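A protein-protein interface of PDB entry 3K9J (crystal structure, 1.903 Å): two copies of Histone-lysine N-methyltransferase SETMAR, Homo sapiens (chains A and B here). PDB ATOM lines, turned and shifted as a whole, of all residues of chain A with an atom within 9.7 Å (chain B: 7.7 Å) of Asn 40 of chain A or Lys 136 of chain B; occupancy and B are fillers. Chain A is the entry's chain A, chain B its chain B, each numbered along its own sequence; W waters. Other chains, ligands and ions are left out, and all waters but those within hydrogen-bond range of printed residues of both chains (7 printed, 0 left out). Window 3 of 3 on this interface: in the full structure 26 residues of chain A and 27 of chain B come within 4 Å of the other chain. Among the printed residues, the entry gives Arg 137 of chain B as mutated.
The side-chain amide nitrogen (ND2) of Asn 40 of chain A sits close to the guanidinium group (NH1) of Arg 46 of chain B, 3.4 Å away.
OE2 of Glu 41 of chain A lies within salt-bridge range of NH2 of Arg 37 of chain B (3.4 Å).
NH2 of Arg 37 of chain A lies within salt-bridge range of OE1 of Glu 41 of chain B, at 3.9 Å.
NH1 of Arg 46 of chain B lies within salt-bridge range of OE1 of Glu 41 of chain A.
The side-chain amide oxygen (OD1) of Asn 40 of chain A lies within hydrogen-bond range of the side-chain amino group (NZ) of Lys 136 of chain B.
O of Arg 46 of chain B is in hydrogen-bond range of N of Ile 139 of chain B (3.0 Å).
The guanidinium group of Arg 46 of chain B is in hydrogen-bond range of the backbone carbonyl oxygen of Arg 137 of chain B, at 2.7 Å.
OE2 of Glu 163 of chain B lies within salt-bridge range of NH2 of Arg 37 of chain B.
OE1 of Gln 129 of chain B lies within hydrogen-bond range of N of Lys 136 of chain B (3.3 Å).
NH2 of Arg 46 of chain B lies within salt-bridge range of OE1 of Glu 163 of chain B.
Among the printed residues, pairs that only touch across the chains: Ser 33 of chain A with Glu 163 of chain B, Leu 36 of chain A with Arg 137 of chain B, Leu 36 of chain A with Glu 163 of chain B, Arg 37 of chain A with Arg 37 of chain B, Arg 37 of chain A with Glu 163 of chain B, Asn 40 of chain A with Arg 137 of chain B and Glu 41 of chain A with Glu 41 of chain B.
Printed residues of chain A within 4 Å of Lys 136 of chain B: Asn 40.
Of the printed residues of chain B, Leu 36 of chain A touches Arg 137 and Glu 163.
Printed residues of chain A within 4 Å of Arg 46 of chain B: Asn 40 and Glu 41.
Printed residues of chain B within 4 Å of Ser 33 of chain A: Glu 163 (3.5 Å).
Of the printed residues of chain B, Glu 41 of chain A touches Arg 37 (3.4 Å), Glu 41 (3.5 Å) and Arg 46 (3.8 Å).
Of the printed residues of chain A, Glu 163 of chain B touches Ser 33, Leu 36 and Arg 37.
Asp 45 of chain B touches none of the printed residues of chain A.
Of the 15 printed residues of chain A, 5 touch a printed residue of chain B.
Along chain B the printed residues that touch a printed residue of chain A span positions 37 to 163.
Among the printed residues, 12 pairs touch across the chains.
Arg 37 of chain B touches its own counterpart, Arg 37 of chain A.
Arg 37 of chain A touches Glu 41 of chain B, and with the chains exchanged Glu 41 of chain A touches Arg 37 of chain B.
Glu 41 of chain B touches its own counterpart, Glu 41 of chain A.
Positions printed for both chains: 37, 41, 42, 43 and 136.
Water W5 lies within hydrogen-bond range of the side-chain carboxylate of Glu 41 of chain B (2.4 Å) and the backbone carbonyl oxygen of Pro 42 of chain A (2.8 Å).
Water W1 lies within hydrogen-bond range of OE2 of Glu 41 of chain A (2.5 Å), O of Glu 41 of chain B (2.7 Å) and NE of Arg 37 of chain B (3.0 Å).
Water W3 lies within hydrogen-bond range of the side-chain carboxylate of Glu 163 of chain B, the guanidinium group of Arg 46 of chain B, the side-chain amide nitrogen of Asn 40 of chain A and the side-chain carboxylate of Glu 41 of chain A.
Water W4 lies within hydrogen-bond range of the side-chain carboxylate of Glu 41 of chain B (2.8 Å), the backbone carbonyl oxygen of Glu 41 of chain A (2.8 Å) and the guanidinium group of Arg 37 of chain A (3.2 Å).
Water W6 lies within hydrogen-bond range of NH1 of Arg 46 of chain B (2.8 Å), OE1 of Glu 41 of chain A (3.0 Å) and O of Pro 42 of chain B (3.0 Å).
Water W2 lies within hydrogen-bond range of O of Leu 36 of chain A (2.9 Å) and NE of Arg 137 of chain B (3.0 Å).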
ATOM      1  N   SER A  32     -12.204  24.740 -14.619  1.00  0.00           N
ATOM      2  CA  SER A  32     -13.172  23.734 -15.005  1.00  0.00           C
ATOM      3  C   SER A  32     -14.154  24.284 -16.026  1.00  0.00           C
ATOM      4  O   SER A  32     -14.506  23.604 -17.005  1.00  0.00           O
ATOM      5  CB  SER A  32     -13.954  23.239 -13.769  1.00  0.00           C
ATOM      6  OG  SER A  32     -15.089  22.479 -14.163  1.00  0.00           O
ATOM      7  N   SER A  33     -14.653  25.496 -15.773  1.00  0.00           N
ATOM      8  CA  SER A  33     -15.612  26.104 -16.686  1.00  0.00           C
ATOM      9  C   SER A  33     -14.978  26.447 -18.042  1.00  0.00           C
ATOM     10  O   SER A  33     -15.627  26.308 -19.067  1.00  0.00           O
ATOM     11  CB  SER A  33     -16.267  27.351 -16.070  1.00  0.00           C
ATOM     12  OG  SER A  33     -17.221  26.958 -15.080  1.00  0.00           O
ATOM     13  N   LEU A  34     -13.735  26.912 -18.041  1.00  0.00           N
ATOM     14  CA  LEU A  34     -13.040  27.195 -19.308  1.00  0.00           C
ATOM     15  C   LEU A  34     -12.818  25.939 -20.151  1.00  0.00           C
ATOM     16  O   LEU A  34     -13.004  25.963 -21.377  1.00  0.00           O
ATOM     17  CB  LEU A  34     -11.718  27.925 -19.071  1.00  0.00           C
ATOM     18  CG  LEU A  34     -11.878  29.320 -18.472  1.00  0.00           C
ATOM     19  CD1 LEU A  34     -10.528  29.921 -18.129  1.00  0.00           C
ATOM     20  CD2 LEU A  34     -12.621  30.224 -19.444  1.00  0.00           C
ATOM     21  N   ILE A  35     -12.412  24.842 -19.517  1.00  0.00           N
ATOM     22  CA  ILE A  35     -12.289  23.571 -20.233  1.00  0.00           C
ATOM     23  C   ILE A  35     -13.605  23.156 -20.880  1.00  0.00           C
ATOM     24  O   ILE A  35     -13.638  22.797 -22.049  1.00  0.00           O
ATOM     25  CB  ILE A  35     -11.885  22.399 -19.279  1.00  0.00           C
ATOM     26  CG1 ILE A  35     -10.491  22.639 -18.707  1.00  0.00           C
ATOM     27  CG2 ILE A  35     -11.920  21.082 -20.015  1.00  0.00           C
ATOM     28  CD1 ILE A  35     -10.164  21.680 -17.579  1.00  0.00           C
ATOM     29  N   LEU A  36     -14.688  23.194 -20.104  1.00  0.00           N
ATOM     30  CA  LEU A  36     -16.009  22.803 -20.580  1.00  0.00           C
ATOM     31  C   LEU A  36     -16.502  23.743 -21.675  1.00  0.00           C
ATOM     32  O   LEU A  36     -17.078  23.312 -22.683  1.00  0.00           O
ATOM     33  CB  LEU A  36     -17.011  22.803 -19.418  1.00  0.00           C
ATOM     34  CG  LEU A  36     -16.764  21.652 -18.445  1.00  0.00           C
ATOM     35  CD1 LEU A  36     -17.420  21.897 -17.082  1.00  0.00           C
ATOM     36  CD2 LEU A  36     -17.264  20.353 -19.093  1.00  0.00           C
ATOM     37  N   ARG A  37     -16.286  25.036 -21.461  1.00  0.00           N
ATOM     38  CA  ARG A  37     -16.721  26.032 -22.419  1.00  0.00           C
ATOM     39  C   ARG A  37     -16.032  25.787 -23.750  1.00  0.00           C
ATOM     40  O   ARG A  37     -16.663  25.788 -24.810  1.00  0.00           O
ATOM     41  CB  ARG A  37     -16.380  27.427 -21.913  1.00  0.00           C
ATOM     42  CG  ARG A  37     -16.717  28.514 -22.931  1.00  0.00           C
ATOM     43  CD  ARG A  37     -16.469  29.903 -22.395  1.00  0.00           C
ATOM     44  NE  ARG A  37     -16.703  30.907 -23.428  1.00  0.00           N
ATOM     45  CZ  ARG A  37     -16.627  32.214 -23.230  1.00  0.00           C
ATOM     46  NH1 ARG A  37     -16.338  32.698 -22.028  1.00  0.00           N
ATOM     47  NH2 ARG A  37     -16.843  33.029 -24.244  1.00  0.00           N
ATOM     48  N   ASN A  38     -14.723  25.568 -23.687  1.00  0.00           N
ATOM     49  CA  ASN A  38     -13.932  25.376 -24.903  1.00  0.00           C
ATOM     50  C   ASN A  38     -14.268  24.076 -25.623  1.00  0.00           C
ATOM     51  O   ASN A  38     -14.187  23.984 -26.854  1.00  0.00           O
ATOM     52  CB  ASN A  38     -12.436  25.405 -24.572  1.00  0.00           C
ATOM     53  CG  ASN A  38     -11.565  25.240 -25.803  1.00  0.00           C
ATOM     54  OD1 ASN A  38     -10.800  24.267 -25.925  1.00  0.00           O
ATOM     55  ND2 ASN A  38     -11.693  26.157 -26.726  1.00  0.00           N
ATOM     56  N   HIS A  39     -14.627  23.061 -24.848  1.00  0.00           N
ATOM     57  CA  HIS A  39     -15.016  21.783 -25.411  1.00  0.00           C
ATOM     58  C   HIS A  39     -16.283  21.964 -26.223  1.00  0.00           C
ATOM     59  O   HIS A  39     -16.405  21.488 -27.346  1.00  0.00           O
ATOM     60  CB  HIS A  39     -15.271  20.772 -24.283  1.00  0.00           C
ATOM     61  CG  HIS A  39     -15.710  19.427 -24.771  1.00  0.00           C
ATOM     62  ND1 HIS A  39     -17.006  18.969 -24.643  1.00  0.00           N
ATOM     63  CD2 HIS A  39     -15.025  18.441 -25.395  1.00  0.00           C
ATOM     64  CE1 HIS A  39     -17.099  17.760 -25.164  1.00  0.00           C
ATOM     65  NE2 HIS A  39     -15.912  17.415 -25.629  1.00  0.00           N
ATOM     66  N   ASN A  40     -17.229  22.690 -25.644  1.00  0.00           N
ATOM     67  CA  ASN A  40     -18.526  22.897 -26.261  1.00  0.00           C
ATOM     68  C   ASN A  40     -18.470  23.901 -27.418  1.00  0.00           C
ATOM     69  O   ASN A  40     -19.068  23.694 -28.470  1.00  0.00           O
ATOM     70  CB  ASN A  40     -19.501  23.390 -25.200  1.00  0.00           C
ATOM     71  CG  ASN A  40     -20.926  23.425 -25.695  1.00  0.00           C
ATOM     72  OD1 ASN A  40     -21.514  22.382 -26.008  1.00  0.00           O
ATOM     73  ND2 ASN A  40     -21.502  24.624 -25.757  1.00  0.00           N
ATOM     74  N   GLU A  41     -17.758  25.000 -27.214  1.00  0.00           N
ATOM     75  CA  GLU A  41     -17.660  26.030 -28.242  1.00  0.00           C
ATOM     76  C   GLU A  41     -16.246  26.596 -28.265  1.00  0.00           C
ATOM     77  O   GLU A  41     -15.945  27.589 -27.595  1.00  0.00           O
ATOM     78  CB  GLU A  41     -18.725  27.129 -28.044  1.00  0.00           C
ATOM     79  CG  GLU A  41     -19.240  27.257 -26.618  1.00  0.00           C
ATOM     80  CD  GLU A  41     -20.253  28.406 -26.436  1.00  0.00           C
ATOM     81  OE1 GLU A  41     -21.295  28.437 -27.152  1.00  0.00           O
ATOM     82  OE2 GLU A  41     -19.989  29.273 -25.567  1.00  0.00           O
ATOM     83  N   PRO A  42     -15.368  25.950 -29.045  1.00  0.00           N
ATOM     84  CA  PRO A  42     -13.950  26.296 -29.100  1.00  0.00           C
ATOM     85  C   PRO A  42     -13.734  27.791 -29.252  1.00  0.00           C
ATOM     86  O   PRO A  42     -14.327  28.417 -30.133  1.00  0.00           O
ATOM     87  CB  PRO A  42     -13.470  25.562 -30.356  1.00  0.00           C
ATOM     88  CG  PRO A  42     -14.351  24.339 -30.411  1.00  0.00           C
ATOM     89  CD  PRO A  42     -15.689  24.784 -29.888  1.00  0.00           C
ATOM     90  N   PHE A  43     -12.882  28.367 -28.416  1.00  0.00           N
ATOM     91  CA  PHE A  43     -12.638  29.793 -28.511  1.00  0.00           C
ATOM     92  C   PHE A  43     -11.159  30.162 -28.502  1.00  0.00           C
ATOM     93  O   PHE A  43     -10.831  31.334 -28.522  1.00  0.00           O
ATOM     94  CB  PHE A  43     -13.368  30.559 -27.383  1.00  0.00           C
ATOM     95  CG  PHE A  43     -12.934  30.155 -25.982  1.00  0.00           C
ATOM     96  CD1 PHE A  43     -13.672  29.236 -25.247  1.00  0.00           C
ATOM     97  CD2 PHE A  43     -11.795  30.701 -25.412  1.00  0.00           C
ATOM     98  CE1 PHE A  43     -13.281  28.859 -23.965  1.00  0.00           C
ATOM     99  CE2 PHE A  43     -11.399  30.347 -24.138  1.00  0.00           C
ATOM    100  CZ  PHE A  43     -12.144  29.416 -23.402  1.00  0.00           C
ATOM    101  N   LYS A 136     -14.572  36.451 -36.139  1.00  0.00           N
ATOM    102  CA  LYS A 136     -15.411  36.461 -34.937  1.00  0.00           C
ATOM    103  C   LYS A 136     -14.768  37.390 -33.898  1.00  0.00           C
ATOM    104  O   LYS A 136     -13.555  37.596 -33.919  1.00  0.00           O
ATOM    105  CB  LYS A 136     -15.570  35.035 -34.392  1.00  0.00           C
ATOM    106  CG  LYS A 136     -16.947  34.728 -33.809  1.00  0.00           C
ATOM    107  CD  LYS A 136     -17.297  33.243 -33.974  1.00  0.00           C
ATOM    108  CE  LYS A 136     -16.343  32.350 -33.178  1.00  0.00           C
ATOM    109  NZ  LYS A 136     -16.350  30.908 -33.593  1.00  0.00           N
ATOM    110  N   ILE A 224      -5.325  24.418 -22.384  1.00  0.00           N
ATOM    111  CA  ILE A 224      -6.208  23.329 -21.992  1.00  0.00           C
ATOM    112  C   ILE A 224      -5.557  22.389 -20.984  1.00  0.00           C
ATOM    113  O   ILE A 224      -6.177  22.022 -19.992  1.00  0.00           O
ATOM    114  CB  ILE A 224      -6.716  22.534 -23.201  1.00  0.00           C
ATOM    115  CG1 ILE A 224      -7.503  23.454 -24.141  1.00  0.00           C
ATOM    116  CG2 ILE A 224      -7.604  21.381 -22.737  1.00  0.00           C
ATOM    117  CD1 ILE A 224      -7.779  22.806 -25.496  1.00  0.00           C
ATOM    118  N   TRP A 227      -5.350  24.313 -17.660  1.00  0.00           N
ATOM    119  CA  TRP A 227      -6.650  24.229 -16.978  1.00  0.00           C
ATOM    120  C   TRP A 227      -6.875  22.836 -16.396  1.00  0.00           C
ATOM    121  O   TRP A 227      -7.352  22.706 -15.256  1.00  0.00           O
ATOM    122  CB  TRP A 227      -7.831  24.581 -17.889  1.00  0.00           C
ATOM    123  CG  TRP A 227      -7.793  25.993 -18.423  1.00  0.00           C
ATOM    124  CD1 TRP A 227      -7.278  27.095 -17.802  1.00  0.00           C
ATOM    125  CD2 TRP A 227      -8.289  26.436 -19.684  1.00  0.00           C
ATOM    126  NE1 TRP A 227      -7.424  28.206 -18.605  1.00  0.00           N
ATOM    127  CE2 TRP A 227      -8.040  27.827 -19.769  1.00  0.00           C
ATOM    128  CE3 TRP A 227      -8.921  25.797 -20.752  1.00  0.00           C
ATOM    129  CZ2 TRP A 227      -8.395  28.590 -20.887  1.00  0.00           C
ATOM    130  CZ3 TRP A 227      -9.260  26.571 -21.882  1.00  0.00           C
ATOM    131  CH2 TRP A 227      -9.011  27.944 -21.922  1.00  0.00           C
ATOM    132  N   ARG B  37     -20.775  38.088 -24.727  1.00  0.00           N
ATOM    133  CA  ARG B  37     -20.738  36.651 -24.948  1.00  0.00           C
ATOM    134  C   ARG B  37     -22.050  36.171 -25.575  1.00  0.00           C
ATOM    135  O   ARG B  37     -22.036  35.394 -26.526  1.00  0.00           O
ATOM    136  CB  ARG B  37     -20.449  35.902 -23.644  1.00  0.00           C
ATOM    137  CG  ARG B  37     -20.559  34.397 -23.829  1.00  0.00           C
ATOM    138  CD  ARG B  37     -20.196  33.624 -22.561  1.00  0.00           C
ATOM    139  NE  ARG B  37     -20.338  32.191 -22.803  1.00  0.00           N
ATOM    140  CZ  ARG B  37     -20.115  31.243 -21.898  1.00  0.00           C
ATOM    141  NH1 ARG B  37     -19.651  31.559 -20.699  1.00  0.00           N
ATOM    142  NH2 ARG B  37     -20.302  29.970 -22.221  1.00  0.00           N
ATOM    143  N   GLU B  41     -22.185  34.254 -28.963  1.00  0.00           N
ATOM    144  CA  GLU B  41     -22.615  32.863 -28.929  1.00  0.00           C
ATOM    145  C   GLU B  41     -23.782  32.716 -27.955  1.00  0.00           C
ATOM    146  O   GLU B  41     -23.569  32.370 -26.797  1.00  0.00           O
ATOM    147  CB  GLU B  41     -21.448  31.982 -28.451  1.00  0.00           C
ATOM    148  CG  GLU B  41     -20.229  31.998 -29.334  1.00  0.00           C
ATOM    149  CD  GLU B  41     -19.007  31.438 -28.630  1.00  0.00           C
ATOM    150  OE1 GLU B  41     -18.680  31.921 -27.522  1.00  0.00           O
ATOM    151  OE2 GLU B  41     -18.381  30.506 -29.180  1.00  0.00           O
ATOM    152  N   PRO B  42     -25.021  32.976 -28.419  1.00  0.00           N
ATOM    153  CA  PRO B  42     -26.159  33.056 -27.495  1.00  0.00           C
ATOM    154  C   PRO B  42     -26.273  31.802 -26.624  1.00  0.00           C
ATOM    155  O   PRO B  42     -26.094  30.676 -27.109  1.00  0.00           O
ATOM    156  CB  PRO B  42     -27.366  33.156 -28.423  1.00  0.00           C
ATOM    157  CG  PRO B  42     -26.801  33.758 -29.711  1.00  0.00           C
ATOM    158  CD  PRO B  42     -25.412  33.206 -29.823  1.00  0.00           C
ATOM    159  N   PHE B  43     -26.584  32.002 -25.350  1.00  0.00           N
ATOM    160  CA  PHE B  43     -26.566  30.893 -24.414  1.00  0.00           C
ATOM    161  C   PHE B  43     -27.697  30.933 -23.400  1.00  0.00           C
ATOM    162  O   PHE B  43     -27.739  30.068 -22.536  1.00  0.00           O
ATOM    163  CB  PHE B  43     -25.223  30.844 -23.676  1.00  0.00           C
ATOM    164  CG  PHE B  43     -24.949  32.069 -22.827  1.00  0.00           C
ATOM    165  CD1 PHE B  43     -24.145  33.096 -23.294  1.00  0.00           C
ATOM    166  CD2 PHE B  43     -25.487  32.182 -21.553  1.00  0.00           C
ATOM    167  CE1 PHE B  43     -23.884  34.219 -22.517  1.00  0.00           C
ATOM    168  CE2 PHE B  43     -25.233  33.303 -20.770  1.00  0.00           C
ATOM    169  CZ  PHE B  43     -24.437  34.323 -21.250  1.00  0.00           C
ATOM    170  N   ASP B  45     -30.728  30.093 -23.401  1.00  0.00           N
ATOM    171  CA  ASP B  45     -31.521  28.869 -23.373  1.00  0.00           C
ATOM    172  C   ASP B  45     -30.836  27.717 -22.638  1.00  0.00           C
ATOM    173  O   ASP B  45     -31.460  26.684 -22.386  1.00  0.00           O
ATOM    174  CB  ASP B  45     -31.881  28.418 -24.789  1.00  0.00           C
ATOM    175  CG  ASP B  45     -30.655  28.064 -25.628  1.00  0.00           C
ATOM    176  OD1 ASP B  45     -29.571  28.654 -25.434  1.00  0.00           O
ATOM    177  OD2 ASP B  45     -30.783  27.176 -26.487  1.00  0.00           O
ATOM    178  N   ARG B  46     -29.556  27.878 -22.306  1.00  0.00           N
ATOM    179  CA  ARG B  46     -28.812  26.804 -21.638  1.00  0.00           C
ATOM    180  C   ARG B  46     -28.697  26.992 -20.131  1.00  0.00           C
ATOM    181  O   ARG B  46     -28.212  26.116 -19.424  1.00  0.00           O
ATOM    182  CB  ARG B  46     -27.400  26.662 -22.247  1.00  0.00           C
ATOM    183  CG  ARG B  46     -27.388  26.271 -23.712  1.00  0.00           C
ATOM    184  CD  ARG B  46     -25.960  26.490 -24.309  1.00  0.00           C
ATOM    185  NE  ARG B  46     -24.989  25.740 -23.522  1.00  0.00           N
ATOM    186  CZ  ARG B  46     -23.696  26.011 -23.457  1.00  0.00           C
ATOM    187  NH1 ARG B  46     -23.198  27.029 -24.153  1.00  0.00           N
ATOM    188  NH2 ARG B  46     -22.909  25.256 -22.697  1.00  0.00           N
ATOM    189  N   VAL B  48     -29.233  27.221 -16.268  1.00  0.00           N
ATOM    190  CA  VAL B  48     -29.960  26.647 -15.137  1.00  0.00           C
ATOM    191  C   VAL B  48     -29.587  27.544 -13.978  1.00  0.00           C
ATOM    192  O   VAL B  48     -28.449  27.963 -13.890  1.00  0.00           O
ATOM    193  CB  VAL B  48     -29.463  25.225 -14.887  1.00  0.00           C
ATOM    194  CG1 VAL B  48     -30.141  24.627 -13.663  1.00  0.00           C
ATOM    195  CG2 VAL B  48     -29.732  24.371 -16.127  1.00  0.00           C
ATOM    196  N   LEU B 125     -33.163  17.053 -14.749  1.00  0.00           N
ATOM    197  CA  LEU B 125     -32.874  17.877 -15.916  1.00  0.00           C
ATOM    198  C   LEU B 125     -32.669  16.961 -17.124  1.00  0.00           C
ATOM    199  O   LEU B 125     -33.180  17.226 -18.212  1.00  0.00           O
ATOM    200  CB  LEU B 125     -31.626  18.744 -15.681  1.00  0.00           C
ATOM    201  CG  LEU B 125     -31.544  20.138 -16.337  1.00  0.00           C
ATOM    202  CD1 LEU B 125     -30.111  20.568 -16.583  1.00  0.00           C
ATOM    203  CD2 LEU B 125     -32.343  20.216 -17.616  1.00  0.00           C
ATOM    204  N   GLN B 129     -34.930  16.904 -20.626  1.00  0.00           N
ATOM    205  CA  GLN B 129     -34.262  17.200 -21.894  1.00  0.00           C
ATOM    206  C   GLN B 129     -34.519  16.149 -22.979  1.00  0.00           C
ATOM    207  O   GLN B 129     -33.927  16.204 -24.054  1.00  0.00           O
ATOM    208  CB  GLN B 129     -32.754  17.400 -21.689  1.00  0.00           C
ATOM    209  CG  GLN B 129     -32.392  18.595 -20.795  1.00  0.00           C
ATOM    210  CD  GLN B 129     -32.225  19.901 -21.559  1.00  0.00           C
ATOM    211  OE1 GLN B 129     -31.477  19.969 -22.530  1.00  0.00           O
ATOM    212  NE2 GLN B 129     -32.908  20.952 -21.107  1.00  0.00           N
ATOM    213  N   LYS B 136     -28.991  20.422 -24.697  1.00  0.00           N
ATOM    214  CA  LYS B 136     -27.732  21.164 -24.744  1.00  0.00           C
ATOM    215  C   LYS B 136     -27.032  21.227 -23.381  1.00  0.00           C
ATOM    216  O   LYS B 136     -27.663  21.053 -22.340  1.00  0.00           O
ATOM    217  CB  LYS B 136     -27.957  22.579 -25.289  1.00  0.00           C
ATOM    218  CG  LYS B 136     -26.669  23.343 -25.544  1.00  0.00           C
ATOM    219  CD  LYS B 136     -25.678  22.510 -26.352  1.00  0.00           C
ATOM    220  CE  LYS B 136     -24.401  23.292 -26.635  1.00  0.00           C
ATOM    221  NZ  LYS B 136     -23.617  22.670 -27.738  1.00  0.00           N
ATOM    222  N   ARG B 137     -25.724  21.474 -23.404  1.00  0.00           N
ATOM    223  CA  ARG B 137     -24.905  21.512 -22.198  1.00  0.00           C
ATOM    224  C   ARG B 137     -25.357  22.638 -21.284  1.00  0.00           C
ATOM    225  O   ARG B 137     -25.362  23.785 -21.698  1.00  0.00           O
ATOM    226  CB  ARG B 137     -23.449  21.755 -22.586  1.00  0.00           C
ATOM    227  CG  ARG B 137     -22.929  20.830 -23.665  1.00  0.00           C
ATOM    228  CD  ARG B 137     -22.565  19.511 -23.054  1.00  0.00           C
ATOM    229  NE  ARG B 137     -21.452  19.652 -22.119  1.00  0.00           N
ATOM    230  CZ  ARG B 137     -21.407  19.068 -20.926  1.00  0.00           C
ATOM    231  NH1 ARG B 137     -22.424  18.315 -20.517  1.00  0.00           N
ATOM    232  NH2 ARG B 137     -20.353  19.248 -20.143  1.00  0.00           N
ATOM    233  N   PRO B 138     -25.731  22.313 -20.035  1.00  0.00           N
ATOM    234  CA  PRO B 138     -26.218  23.323 -19.096  1.00  0.00           C
ATOM    235  C   PRO B 138     -25.098  24.251 -18.641  1.00  0.00           C
ATOM    236  O   PRO B 138     -23.929  23.869 -18.572  1.00  0.00           O
ATOM    237  CB  PRO B 138     -26.710  22.491 -17.896  1.00  0.00           C
ATOM    238  CG  PRO B 138     -26.786  21.078 -18.397  1.00  0.00           C
ATOM    239  CD  PRO B 138     -25.738  20.964 -19.442  1.00  0.00           C
ATOM    240  N   ILE B 139     -25.473  25.488 -18.354  1.00  0.00           N
ATOM    241  CA  ILE B 139     -24.581  26.449 -17.732  1.00  0.00           C
ATOM    242  C   ILE B 139     -25.259  26.915 -16.454  1.00  0.00           C
ATOM    243  O   ILE B 139     -26.412  27.321 -16.488  1.00  0.00           O
ATOM    244  CB  ILE B 139     -24.408  27.663 -18.629  1.00  0.00           C
ATOM    245  CG1 ILE B 139     -23.785  27.250 -19.958  1.00  0.00           C
ATOM    246  CG2 ILE B 139     -23.567  28.732 -17.928  1.00  0.00           C
ATOM    247  CD1 ILE B 139     -23.686  28.427 -20.962  1.00  0.00           C
ATOM    248  N   GLU B 163     -20.729  23.967 -16.861  1.00  0.00           N
ATOM    249  CA  GLU B 163     -20.048  25.225 -16.914  1.00  0.00           C
ATOM    250  C   GLU B 163     -20.748  26.127 -15.901  1.00  0.00           C
ATOM    251  O   GLU B 163     -21.925  25.911 -15.611  1.00  0.00           O
ATOM    252  CB  GLU B 163     -20.287  25.782 -18.311  1.00  0.00           C
ATOM    253  CG  GLU B 163     -19.114  26.295 -19.009  1.00  0.00           C
ATOM    254  CD  GLU B 163     -19.530  26.968 -20.308  1.00  0.00           C
ATOM    255  OE1 GLU B 163     -19.834  26.242 -21.287  1.00  0.00           O
ATOM    256  OE2 GLU B 163     -19.579  28.212 -20.324  1.00  0.00           O
HETATM  257  O   HOH W   1     -21.734  31.055 -25.234  1.00  0.00           O
HETATM  258  O   HOH W   2     -19.090  21.289 -22.840  1.00  0.00           O
HETATM  259  O   HOH W   3     -20.293  26.718 -23.927  1.00  0.00           O
HETATM  260  O   HOH W   4     -16.973  29.959 -26.461  1.00  0.00           O
HETATM  261  O   HOH W   5     -16.095  30.557 -30.050  1.00  0.00           O
HETATM  262  O   HOH W   6     -24.161  28.488 -26.387  1.00  0.00           O
HETATM  263  O   HOH W   7     -18.066  34.468 -26.969  1.00  0.00           O
